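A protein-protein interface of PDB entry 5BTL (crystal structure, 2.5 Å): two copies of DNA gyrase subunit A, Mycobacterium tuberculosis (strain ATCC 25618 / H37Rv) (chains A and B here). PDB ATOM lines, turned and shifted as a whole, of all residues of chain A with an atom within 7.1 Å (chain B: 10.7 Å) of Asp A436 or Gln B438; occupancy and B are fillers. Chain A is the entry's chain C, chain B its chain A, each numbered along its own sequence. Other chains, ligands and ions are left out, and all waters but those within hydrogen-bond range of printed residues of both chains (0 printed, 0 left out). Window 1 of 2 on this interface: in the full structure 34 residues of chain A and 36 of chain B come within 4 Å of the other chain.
The side-chain amide nitrogen of Gln A438 sits at hydrogen-bond distance from the backbone carbonyl oxygen of Asp B436 (3.0 Å). The backbone NH of Leu B439 lies within hydrogen-bond range of the backbone carbonyl oxygen of Leu A435 (3.4 Å). The backbone carbonyl oxygen (O) of Met B437 is in hydrogen-bond range of the backbone NH (N) of Leu A439, at 2.8 Å. N of Leu B439 is in hydrogen-bond range of O of Met A437, 2.8 Å away. The backbone carbonyl oxygen of Leu A435 sits at hydrogen-bond distance from the backbone NH of Arg B440, at 2.9 Å. NE2 of Gln B438 lies within hydrogen-bond range of O of Asp A436 (3.0 Å). The guanidinium group (NE) of Arg B440 is in salt-bridge range of the side-chain carboxylate (OD1) of Asp A436 (2.4 Å).
Leu B439 touches Ile A434. Leu A435 touches Gln B438 (O to CB, 3.9 Å). O of Met A437 touches CA of Gln B438 (3.3 Å). CB of Gln A438 touches O of Leu B435, 3.9 Å away. CA of Gln A438 touches O of Met B437, at 3.3 Å. Leu A439 touches Ile B407 (O to CG2, 3.5 Å). CD1 of Leu A439 touches O of Ile B434 (3.5 Å). O of Leu B435 touches N of Leu A439 (3.6 Å). CD2 of Leu A439 touches CD2 of Leu B439, at 3.4 Å.
Of chain B, only Gln B438 (3.0 Å) and Arg B440 (2.4 Å) come within 4 Å of Asp A436. Printed residues of chain A within 4 Å of Gln B438: Leu A435, Asp A436 and Met A437. No residue of chain B comes within 4 Å of Gln A432. No residue of chain B comes within 4 Å of Ala A433. Met A437 touches just these residues of chain B: Gln B438 and Leu B439. Of chain B, only Leu B435, Asp B436 and Met B437 come within 4 Å of Gln A438. Of the printed residues of chain B, Leu A439 touches Ile B407, Ile B434, Leu B435, Met B437 and Leu B439. Of the printed residues of chain A, Leu B435 touches Gln A438 and Leu A439. Printed residues of chain A within 4 Å of Met B437: Gln A438 (3.3 Å) and Leu A439 (2.8 Å). Of the printed residues of chain A, Ile B407 touches Leu A439 (3.5 Å). Glu B446 touches none of the printed residues of chain A. Leu B442 touches none of the printed residues of chain A.
Printed residues of chain A that touch a printed residue of chain B: Ile A434, Leu A435, Asp A436, Met A437, Gln A438 and Leu A439. Hydrophobic or aromatic side chains of chain A within 4 Å of the printed part of chain B: Leu A439. Of the 24 printed residues of chain B, 8 touch a printed residue of chain A.
Leu A435 touches Gln B438, and with the chains exchanged Gln A438 touches Leu B435. Leu A435 touches Leu B439, and with the chains exchanged Leu A439 touches Leu B435. Met A437 touches Gln B438, and with the chains exchanged Gln A438 touches Met B437. Leu B439 touches its own counterpart, Leu A439. Positions printed for both chains: 431, 432, 433, 434, 435, 436, 437, 438, 439 and 441.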
ATOM      1  N   ILE A 429       4.225   9.396  -2.813  1.00  0.00           N
ATOM      2  CA  ILE A 429       3.197   9.955  -1.943  1.00  0.00           C
ATOM      3  C   ILE A 429       2.023   8.987  -1.894  1.00  0.00           C
ATOM      4  O   ILE A 429       1.495   8.672  -0.827  1.00  0.00           O
ATOM      5  CB  ILE A 429       2.718  11.342  -2.428  1.00  0.00           C
ATOM      6  CG1 ILE A 429       3.849  12.372  -2.344  1.00  0.00           C
ATOM      7  CG2 ILE A 429       1.527  11.831  -1.604  1.00  0.00           C
ATOM      8  CD1 ILE A 429       4.735  12.441  -3.579  1.00  0.00           C
ATOM      9  N   GLN A 430       1.629   8.522  -3.072  1.00  0.00           N
ATOM     10  CA  GLN A 430       0.538   7.574  -3.213  1.00  0.00           C
ATOM     11  C   GLN A 430       0.898   6.247  -2.552  1.00  0.00           C
ATOM     12  O   GLN A 430       0.083   5.649  -1.850  1.00  0.00           O
ATOM     13  CB  GLN A 430       0.223   7.368  -4.692  1.00  0.00           C
ATOM     14  CG  GLN A 430      -0.601   8.470  -5.327  1.00  0.00           C
ATOM     15  CD  GLN A 430      -0.648   8.353  -6.838  1.00  0.00           C
ATOM     16  OE1 GLN A 430       0.385   8.393  -7.505  1.00  0.00           O
ATOM     17  NE2 GLN A 430      -1.847   8.192  -7.385  1.00  0.00           N
ATOM     18  N   ALA A 431       2.125   5.792  -2.787  1.00  0.00           N
ATOM     19  CA  ALA A 431       2.613   4.545  -2.204  1.00  0.00           C
ATOM     20  C   ALA A 431       2.611   4.632  -0.682  1.00  0.00           C
ATOM     21  O   ALA A 431       2.312   3.657   0.007  1.00  0.00           O
ATOM     22  CB  ALA A 431       4.009   4.229  -2.715  1.00  0.00           C
ATOM     23  N   GLN A 432       2.958   5.807  -0.166  1.00  0.00           N
ATOM     24  CA  GLN A 432       2.944   6.049   1.272  1.00  0.00           C
ATOM     25  C   GLN A 432       1.526   5.911   1.816  1.00  0.00           C
ATOM     26  O   GLN A 432       1.319   5.393   2.912  1.00  0.00           O
ATOM     27  CB  GLN A 432       3.494   7.444   1.585  1.00  0.00           C
ATOM     28  CG  GLN A 432       3.803   7.687   3.055  1.00  0.00           C
ATOM     29  CD  GLN A 432       4.950   6.833   3.558  1.00  0.00           C
ATOM     30  OE1 GLN A 432       4.741   5.770   4.143  1.00  0.00           O
ATOM     31  NE2 GLN A 432       6.175   7.293   3.325  1.00  0.00           N
ATOM     32  N   ALA A 433       0.553   6.369   1.035  1.00  0.00           N
ATOM     33  CA  ALA A 433      -0.848   6.316   1.439  1.00  0.00           C
ATOM     34  C   ALA A 433      -1.343   4.878   1.516  1.00  0.00           C
ATOM     35  O   ALA A 433      -2.145   4.538   2.385  1.00  0.00           O
ATOM     36  CB  ALA A 433      -1.706   7.121   0.478  1.00  0.00           C
ATOM     37  N   ILE A 434      -0.870   4.039   0.598  1.00  0.00           N
ATOM     38  CA  ILE A 434      -1.205   2.621   0.623  1.00  0.00           C
ATOM     39  C   ILE A 434      -0.694   2.009   1.922  1.00  0.00           C
ATOM     40  O   ILE A 434      -1.397   1.238   2.574  1.00  0.00           O
ATOM     41  CB  ILE A 434      -0.604   1.868  -0.584  1.00  0.00           C
ATOM     42  CG1 ILE A 434      -1.191   2.402  -1.892  1.00  0.00           C
ATOM     43  CG2 ILE A 434      -0.854   0.364  -0.468  1.00  0.00           C
ATOM     44  CD1 ILE A 434      -0.459   1.933  -3.137  1.00  0.00           C
ATOM     45  N   LEU A 435       0.531   2.364   2.292  1.00  0.00           N
ATOM     46  CA  LEU A 435       1.134   1.873   3.526  1.00  0.00           C
ATOM     47  C   LEU A 435       0.350   2.360   4.743  1.00  0.00           C
ATOM     48  O   LEU A 435       0.143   1.609   5.696  1.00  0.00           O
ATOM     49  CB  LEU A 435       2.597   2.316   3.621  1.00  0.00           C
ATOM     50  CG  LEU A 435       3.596   1.548   2.748  1.00  0.00           C
ATOM     51  CD1 LEU A 435       4.948   2.244   2.740  1.00  0.00           C
ATOM     52  CD2 LEU A 435       3.747   0.107   3.216  1.00  0.00           C
ATOM     53  N   ASP A 436      -0.095   3.614   4.698  1.00  0.00           N
ATOM     54  CA  ASP A 436      -0.826   4.214   5.813  1.00  0.00           C
ATOM     55  C   ASP A 436      -2.258   3.697   5.908  1.00  0.00           C
ATOM     56  O   ASP A 436      -2.977   4.017   6.855  1.00  0.00           O
ATOM     57  CB  ASP A 436      -0.854   5.739   5.678  1.00  0.00           C
ATOM     58  CG  ASP A 436       0.531   6.353   5.647  1.00  0.00           C
ATOM     59  OD1 ASP A 436       1.481   5.702   6.124  1.00  0.00           O
ATOM     60  OD2 ASP A 436       0.667   7.490   5.148  1.00  0.00           O
ATOM     61  N   MET A 437      -2.673   2.905   4.926  1.00  0.00           N
ATOM     62  CA  MET A 437      -4.036   2.391   4.882  1.00  0.00           C
ATOM     63  C   MET A 437      -4.290   1.426   6.037  1.00  0.00           C
ATOM     64  O   MET A 437      -3.446   0.589   6.353  1.00  0.00           O
ATOM     65  CB  MET A 437      -4.297   1.698   3.543  1.00  0.00           C
ATOM     66  CG  MET A 437      -5.766   1.609   3.170  1.00  0.00           C
ATOM     67  SD  MET A 437      -6.114   0.485   1.801  1.00  0.00           S
ATOM     68  CE  MET A 437      -4.802   0.903   0.654  1.00  0.00           C
ATOM     69  N   GLN A 438      -5.458   1.547   6.661  1.00  0.00           N
ATOM     70  CA  GLN A 438      -5.835   0.671   7.768  1.00  0.00           C
ATOM     71  C   GLN A 438      -6.470  -0.611   7.245  1.00  0.00           C
ATOM     72  O   GLN A 438      -7.004  -0.636   6.135  1.00  0.00           O
ATOM     73  CB  GLN A 438      -6.807   1.377   8.712  1.00  0.00           C
ATOM     74  CG  GLN A 438      -6.199   2.517   9.504  1.00  0.00           C
ATOM     75  CD  GLN A 438      -7.227   3.236  10.358  1.00  0.00           C
ATOM     76  OE1 GLN A 438      -8.256   3.692   9.859  1.00  0.00           O
ATOM     77  NE2 GLN A 438      -6.956   3.333  11.655  1.00  0.00           N
ATOM     78  N   LEU A 439      -6.409  -1.674   8.043  1.00  0.00           N
ATOM     79  CA  LEU A 439      -7.048  -2.930   7.673  1.00  0.00           C
ATOM     80  C   LEU A 439      -8.564  -2.763   7.581  1.00  0.00           C
ATOM     81  O   LEU A 439      -9.237  -3.549   6.914  1.00  0.00           O
ATOM     82  CB  LEU A 439      -6.696  -4.030   8.679  1.00  0.00           C
ATOM     83  CG  LEU A 439      -5.213  -4.402   8.792  1.00  0.00           C
ATOM     84  CD1 LEU A 439      -5.008  -5.477   9.847  1.00  0.00           C
ATOM     85  CD2 LEU A 439      -4.655  -4.864   7.456  1.00  0.00           C
ATOM     86  N   ARG A 441     -10.024  -0.477   5.886  1.00  0.00           N
ATOM     87  CA  ARG A 441     -10.376  -0.036   4.545  1.00  0.00           C
ATOM     88  C   ARG A 441     -10.335  -1.184   3.539  1.00  0.00           C
ATOM     89  O   ARG A 441     -10.605  -0.985   2.355  1.00  0.00           O
ATOM     90  CB  ARG A 441      -9.423   1.077   4.092  1.00  0.00           C
ATOM     91  CG  ARG A 441      -9.621   2.420   4.790  1.00  0.00           C
ATOM     92  CD  ARG A 441      -8.699   3.478   4.190  1.00  0.00           C
ATOM     93  NE  ARG A 441      -8.619   4.693   4.998  1.00  0.00           N
ATOM     94  CZ  ARG A 441      -7.717   5.655   4.817  1.00  0.00           C
ATOM     95  NH1 ARG A 441      -6.808   5.552   3.856  1.00  0.00           N
ATOM     96  NH2 ARG A 441      -7.718   6.724   5.604  1.00  0.00           N
ATOM     97  N   LEU B 393      -2.849  -8.199  18.939  1.00  0.00           N
ATOM     98  CA  LEU B 393      -2.077  -8.048  17.711  1.00  0.00           C
ATOM     99  C   LEU B 393      -1.274  -9.307  17.395  1.00  0.00           C
ATOM    100  O   LEU B 393      -1.220  -9.741  16.246  1.00  0.00           O
ATOM    101  CB  LEU B 393      -1.135  -6.846  17.813  1.00  0.00           C
ATOM    102  CG  LEU B 393      -1.752  -5.487  18.158  1.00  0.00           C
ATOM    103  CD1 LEU B 393      -0.726  -4.385  17.955  1.00  0.00           C
ATOM    104  CD2 LEU B 393      -2.999  -5.200  17.342  1.00  0.00           C
ATOM    105  N   ALA B 396      -3.302 -11.937  15.916  1.00  0.00           N
ATOM    106  CA  ALA B 396      -3.588 -11.609  14.525  1.00  0.00           C
ATOM    107  C   ALA B 396      -2.418 -11.997  13.625  1.00  0.00           C
ATOM    108  O   ALA B 396      -2.618 -12.541  12.540  1.00  0.00           O
ATOM    109  CB  ALA B 396      -3.902 -10.125  14.384  1.00  0.00           C
ATOM    110  N   LEU B 397      -1.200 -11.725  14.082  1.00  0.00           N
ATOM    111  CA  LEU B 397      -0.001 -12.033  13.306  1.00  0.00           C
ATOM    112  C   LEU B 397       0.181 -13.539  13.123  1.00  0.00           C
ATOM    113  O   LEU B 397       0.592 -13.995  12.056  1.00  0.00           O
ATOM    114  CB  LEU B 397       1.239 -11.436  13.975  1.00  0.00           C
ATOM    115  CG  LEU B 397       1.316  -9.908  14.057  1.00  0.00           C
ATOM    116  CD1 LEU B 397       2.570  -9.475  14.798  1.00  0.00           C
ATOM    117  CD2 LEU B 397       1.274  -9.274  12.672  1.00  0.00           C
ATOM    118  N   LEU B 400      -2.298 -14.446  10.441  1.00  0.00           N
ATOM    119  CA  LEU B 400      -2.407 -13.280   9.567  1.00  0.00           C
ATOM    120  C   LEU B 400      -3.174 -13.555   8.274  1.00  0.00           C
ATOM    121  O   LEU B 400      -3.973 -12.726   7.836  1.00  0.00           O
ATOM    122  CB  LEU B 400      -1.008 -12.759   9.227  1.00  0.00           C
ATOM    123  CG  LEU B 400      -0.926 -11.487   8.380  1.00  0.00           C
ATOM    124  CD1 LEU B 400      -1.732 -10.355   9.001  1.00  0.00           C
ATOM    125  CD2 LEU B 400       0.524 -11.075   8.197  1.00  0.00           C
ATOM    126  N   VAL B 403      -6.897 -13.491   9.095  1.00  0.00           N
ATOM    127  CA  VAL B 403      -7.405 -12.179   9.486  1.00  0.00           C
ATOM    128  C   VAL B 403      -7.883 -11.364   8.284  1.00  0.00           C
ATOM    129  O   VAL B 403      -8.982 -10.810   8.299  1.00  0.00           O
ATOM    130  CB  VAL B 403      -6.323 -11.373  10.252  1.00  0.00           C
ATOM    131  CG1 VAL B 403      -6.737  -9.911  10.431  1.00  0.00           C
ATOM    132  CG2 VAL B 403      -6.046 -12.007  11.600  1.00  0.00           C
ATOM    133  N   ILE B 404      -7.055 -11.295   7.249  1.00  0.00           N
ATOM    134  CA  ILE B 404      -7.370 -10.493   6.073  1.00  0.00           C
ATOM    135  C   ILE B 404      -8.583 -11.027   5.317  1.00  0.00           C
ATOM    136  O   ILE B 404      -9.490 -10.266   4.980  1.00  0.00           O
ATOM    137  CB  ILE B 404      -6.165 -10.429   5.115  1.00  0.00           C
ATOM    138  CG1 ILE B 404      -4.971  -9.789   5.830  1.00  0.00           C
ATOM    139  CG2 ILE B 404      -6.524  -9.658   3.837  1.00  0.00           C
ATOM    140  CD1 ILE B 404      -3.696  -9.777   5.025  1.00  0.00           C
ATOM    141  N   ILE B 407     -11.932 -10.040   7.002  1.00  0.00           N
ATOM    142  CA  ILE B 407     -12.308  -8.634   6.902  1.00  0.00           C
ATOM    143  C   ILE B 407     -12.871  -8.321   5.518  1.00  0.00           C
ATOM    144  O   ILE B 407     -13.795  -7.519   5.382  1.00  0.00           O
ATOM    145  CB  ILE B 407     -11.103  -7.711   7.199  1.00  0.00           C
ATOM    146  CG1 ILE B 407     -10.638  -7.908   8.645  1.00  0.00           C
ATOM    147  CG2 ILE B 407     -11.467  -6.244   6.952  1.00  0.00           C
ATOM    148  CD1 ILE B 407      -9.365  -7.164   9.003  1.00  0.00           C
ATOM    149  N   ALA B 431      -9.923  -6.312  19.033  1.00  0.00           N
ATOM    150  CA  ALA B 431     -10.359  -6.464  17.653  1.00  0.00           C
ATOM    151  C   ALA B 431     -10.403  -5.109  16.964  1.00  0.00           C
ATOM    152  O   ALA B 431     -10.039  -4.983  15.794  1.00  0.00           O
ATOM    153  CB  ALA B 431     -11.721  -7.138  17.594  1.00  0.00           C
ATOM    154  N   GLN B 432     -10.847  -4.095  17.699  1.00  0.00           N
ATOM    155  CA  GLN B 432     -10.880  -2.734  17.184  1.00  0.00           C
ATOM    156  C   GLN B 432      -9.468  -2.246  16.883  1.00  0.00           C
ATOM    157  O   GLN B 432      -9.239  -1.549  15.894  1.00  0.00           O
ATOM    158  CB  GLN B 432     -11.567  -1.799  18.182  1.00  0.00           C
ATOM    159  CG  GLN B 432     -11.897  -0.429  17.618  1.00  0.00           C
ATOM    160  CD  GLN B 432     -12.928  -0.494  16.512  1.00  0.00           C
ATOM    161  OE1 GLN B 432     -12.582  -0.518  15.329  1.00  0.00           O
ATOM    162  NE2 GLN B 432     -14.202  -0.530  16.886  1.00  0.00           N
ATOM    163  N   ALA B 433      -8.523  -2.622  17.740  1.00  0.00           N
ATOM    164  CA  ALA B 433      -7.131  -2.224  17.570  1.00  0.00           C
ATOM    165  C   ALA B 433      -6.536  -2.896  16.339  1.00  0.00           C
ATOM    166  O   ALA B 433      -5.747  -2.293  15.611  1.00  0.00           O
ATOM    167  CB  ALA B 433      -6.325  -2.569  18.812  1.00  0.00           C
ATOM    168  N   ILE B 434      -6.915  -4.150  16.114  1.00  0.00           N
ATOM    169  CA  ILE B 434      -6.501  -4.872  14.917  1.00  0.00           C
ATOM    170  C   ILE B 434      -7.049  -4.164  13.684  1.00  0.00           C
ATOM    171  O   ILE B 434      -6.350  -4.006  12.685  1.00  0.00           O
ATOM    172  CB  ILE B 434      -6.980  -6.343  14.939  1.00  0.00           C
ATOM    173  CG1 ILE B 434      -6.307  -7.102  16.085  1.00  0.00           C
ATOM    174  CG2 ILE B 434      -6.667  -7.037  13.613  1.00  0.00           C
ATOM    175  CD1 ILE B 434      -6.919  -8.460  16.378  1.00  0.00           C
ATOM    176  N   LEU B 435      -8.306  -3.737  13.767  1.00  0.00           N
ATOM    177  CA  LEU B 435      -8.959  -3.040  12.665  1.00  0.00           C
ATOM    178  C   LEU B 435      -8.257  -1.726  12.339  1.00  0.00           C
ATOM    179  O   LEU B 435      -8.088  -1.377  11.170  1.00  0.00           O
ATOM    180  CB  LEU B 435     -10.426  -2.777  13.006  1.00  0.00           C
ATOM    181  CG  LEU B 435     -11.381  -3.967  12.899  1.00  0.00           C
ATOM    182  CD1 LEU B 435     -12.721  -3.617  13.519  1.00  0.00           C
ATOM    183  CD2 LEU B 435     -11.561  -4.390  11.448  1.00  0.00           C
ATOM    184  N   ASP B 436      -7.847  -1.003  13.376  1.00  0.00           N
ATOM    185  CA  ASP B 436      -7.184   0.285  13.196  1.00  0.00           C
ATOM    186  C   ASP B 436      -5.735   0.125  12.741  1.00  0.00           C
ATOM    187  O   ASP B 436      -5.063   1.111  12.440  1.00  0.00           O
ATOM    188  CB  ASP B 436      -7.229   1.095  14.494  1.00  0.00           C
ATOM    189  CG  ASP B 436      -8.644   1.378  14.957  1.00  0.00           C
ATOM    190  OD1 ASP B 436      -9.568   1.335  14.117  1.00  0.00           O
ATOM    191  OD2 ASP B 436      -8.832   1.651  16.163  1.00  0.00           O
ATOM    192  N   MET B 437      -5.254  -1.115  12.689  1.00  0.00           N
ATOM    193  CA  MET B 437      -3.867  -1.376  12.320  1.00  0.00           C
ATOM    194  C   MET B 437      -3.594  -0.993  10.872  1.00  0.00           C
ATOM    195  O   MET B 437      -4.393  -1.281   9.982  1.00  0.00           O
ATOM    196  CB  MET B 437      -3.526  -2.852  12.519  1.00  0.00           C
ATOM    197  CG  MET B 437      -2.041  -3.122  12.680  1.00  0.00           C
ATOM    198  SD  MET B 437      -1.603  -4.861  12.492  1.00  0.00           S
ATOM    199  CE  MET B 437      -2.918  -5.668  13.405  1.00  0.00           C
ATOM    200  N   GLN B 438      -2.455  -0.347  10.644  1.00  0.00           N
ATOM    201  CA  GLN B 438      -2.050   0.055   9.302  1.00  0.00           C
ATOM    202  C   GLN B 438      -1.276  -1.056   8.600  1.00  0.00           C
ATOM    203  O   GLN B 438      -0.662  -1.903   9.249  1.00  0.00           O
ATOM    204  CB  GLN B 438      -1.199   1.325   9.366  1.00  0.00           C
ATOM    205  CG  GLN B 438      -1.970   2.563   9.792  1.00  0.00           C
ATOM    206  CD  GLN B 438      -1.081   3.785   9.933  1.00  0.00           C
ATOM    207  OE1 GLN B 438      -0.087   3.765  10.659  1.00  0.00           O
ATOM    208  NE2 GLN B 438      -1.433   4.856   9.231  1.00  0.00           N
ATOM    209  N   LEU B 439      -1.305  -1.041   7.270  1.00  0.00           N
ATOM    210  CA  LEU B 439      -0.523  -1.979   6.470  1.00  0.00           C
ATOM    211  C   LEU B 439       0.969  -1.746   6.691  1.00  0.00           C
ATOM    212  O   LEU B 439       1.797  -2.601   6.369  1.00  0.00           O
ATOM    213  CB  LEU B 439      -0.867  -1.850   4.984  1.00  0.00           C
ATOM    214  CG  LEU B 439      -2.314  -2.159   4.585  1.00  0.00           C
ATOM    215  CD1 LEU B 439      -2.507  -1.968   3.091  1.00  0.00           C
ATOM    216  CD2 LEU B 439      -2.716  -3.569   4.993  1.00  0.00           C
ATOM    217  N   ARG B 440       1.298  -0.574   7.228  1.00  0.00           N
ATOM    218  CA  ARG B 440       2.662  -0.236   7.621  1.00  0.00           C
ATOM    219  C   ARG B 440       3.296  -1.356   8.438  1.00  0.00           C
ATOM    220  O   ARG B 440       4.412  -1.793   8.162  1.00  0.00           O
ATOM    221  CB  ARG B 440       2.649   1.042   8.466  1.00  0.00           C
ATOM    222  CG  ARG B 440       2.652   2.349   7.697  1.00  0.00           C
ATOM    223  CD  ARG B 440       2.785   3.525   8.652  1.00  0.00           C
ATOM    224  NE  ARG B 440       2.797   4.809   7.955  1.00  0.00           N
ATOM    225  CZ  ARG B 440       3.193   5.958   8.496  1.00  0.00           C
ATOM    226  NH1 ARG B 440       3.610   6.001   9.755  1.00  0.00           N
ATOM    227  NH2 ARG B 440       3.158   7.073   7.778  1.00  0.00           N
ATOM    228  N   ARG B 441       2.556  -1.819   9.441  1.00  0.00           N
ATOM    229  CA  ARG B 441       3.080  -2.750  10.434  1.00  0.00           C
ATOM    230  C   ARG B 441       3.115  -4.215   9.992  1.00  0.00           C
ATOM    231  O   ARG B 441       3.493  -5.085  10.776  1.00  0.00           O
ATOM    232  CB  ARG B 441       2.280  -2.622  11.733  1.00  0.00           C
ATOM    233  CG  ARG B 441       2.596  -1.343  12.498  1.00  0.00           C
ATOM    234  CD  ARG B 441       1.897  -1.284  13.846  1.00  0.00           C
ATOM    235  NE  ARG B 441       0.551  -0.730  13.750  1.00  0.00           N
ATOM    236  CZ  ARG B 441      -0.204  -0.415  14.799  1.00  0.00           C
ATOM    237  NH1 ARG B 441       0.253  -0.597  16.031  1.00  0.00           N
ATOM    238  NH2 ARG B 441      -1.418   0.086  14.615  1.00  0.00           N
ATOM    239  N   LEU B 442       2.738  -4.491   8.747  1.00  0.00           N
ATOM    240  CA  LEU B 442       2.742  -5.865   8.249  1.00  0.00           C
ATOM    241  C   LEU B 442       4.101  -6.238   7.659  1.00  0.00           C
ATOM    242  O   LEU B 442       4.314  -7.379   7.247  1.00  0.00           O
ATOM    243  CB  LEU B 442       1.642  -6.066   7.202  1.00  0.00           C
ATOM    244  CG  LEU B 442       0.193  -5.928   7.685  1.00  0.00           C
ATOM    245  CD1 LEU B 442      -0.775  -6.211   6.547  1.00  0.00           C
ATOM    246  CD2 LEU B 442      -0.099  -6.848   8.866  1.00  0.00           C
ATOM    247  N   ALA B 443       5.017  -5.275   7.622  1.00  0.00           N
ATOM    248  CA  ALA B 443       6.386  -5.541   7.195  1.00  0.00           C
ATOM    249  C   ALA B 443       7.080  -6.410   8.241  1.00  0.00           C
ATOM    250  O   ALA B 443       6.679  -6.425   9.403  1.00  0.00           O
ATOM    251  CB  ALA B 443       7.144  -4.243   6.981  1.00  0.00           C
ATOM    252  N   ALA B 444       8.117  -7.130   7.820  1.00  0.00           N
ATOM    253  CA  ALA B 444       8.795  -8.101   8.681  1.00  0.00           C
ATOM    254  C   ALA B 444       9.257  -7.515  10.014  1.00  0.00           C
ATOM    255  O   ALA B 444       8.882  -8.012  11.076  1.00  0.00           O
ATOM    256  CB  ALA B 444       9.982  -8.698   7.949  1.00  0.00           C
ATOM    257  N   GLU B 446       8.430  -4.829  11.438  1.00  0.00           N
ATOM    258  CA  GLU B 446       7.326  -4.245  12.191  1.00  0.00           C
ATOM    259  C   GLU B 446       6.532  -5.323  12.918  1.00  0.00           C
ATOM    260  O   GLU B 446       6.075  -5.111  14.040  1.00  0.00           O
ATOM    261  CB  GLU B 446       6.406  -3.448  11.269  1.00  0.00           C
ATOM    262  CG  GLU B 446       7.062  -2.228  10.637  1.00  0.00           C
ATOM    263  CD  GLU B 446       7.446  -1.171  11.659  1.00  0.00           C
ATOM    264  OE1 GLU B 446       6.950  -1.236  12.803  1.00  0.00           O
ATOM    265  OE2 GLU B 446       8.249  -0.279  11.320  1.00  0.00           O
ATOM    266  N   ARG B 447       6.367  -6.477  12.279  1.00  0.00           N
ATOM    267  CA  ARG B 447       5.742  -7.616  12.936  1.00  0.00           C
ATOM    268  C   ARG B 447       6.580  -8.041  14.136  1.00  0.00           C
ATOM    269  O   ARG B 447       6.045  -8.367  15.194  1.00  0.00           O
ATOM    270  CB  ARG B 447       5.563  -8.781  11.957  1.00  0.00           C
ATOM    271  CG  ARG B 447       4.511  -8.515  10.889  1.00  0.00           C
ATOM    272  CD  ARG B 447       4.221  -9.739  10.033  1.00  0.00           C
ATOM    273  NE  ARG B 447       5.098  -9.830   8.864  1.00  0.00           N
ATOM    274  CZ  ARG B 447       6.137 -10.654   8.743  1.00  0.00           C
ATOM    275  NH1 ARG B 447       6.477 -11.484   9.725  1.00  0.00           N
ATOM    276  NH2 ARG B 447       6.853 -10.643   7.627  1.00  0.00           N
ATOM    277  N   ILE B 450       6.241  -5.585  17.075  1.00  0.00           N
ATOM    278  CA  ILE B 450       5.044  -5.842  17.871  1.00  0.00           C
ATOM    279  C   ILE B 450       5.318  -6.932  18.908  1.00  0.00           C
ATOM    280  O   ILE B 450       4.948  -6.794  20.076  1.00  0.00           O
ATOM    281  CB  ILE B 450       3.851  -6.249  16.975  1.00  0.00           C
ATOM    282  CG1 ILE B 450       3.445  -5.076  16.081  1.00  0.00           C
ATOM    283  CG2 ILE B 450       2.655  -6.687  17.822  1.00  0.00           C
ATOM    284  CD1 ILE B 450       2.455  -5.432  14.991  1.00  0.00           C
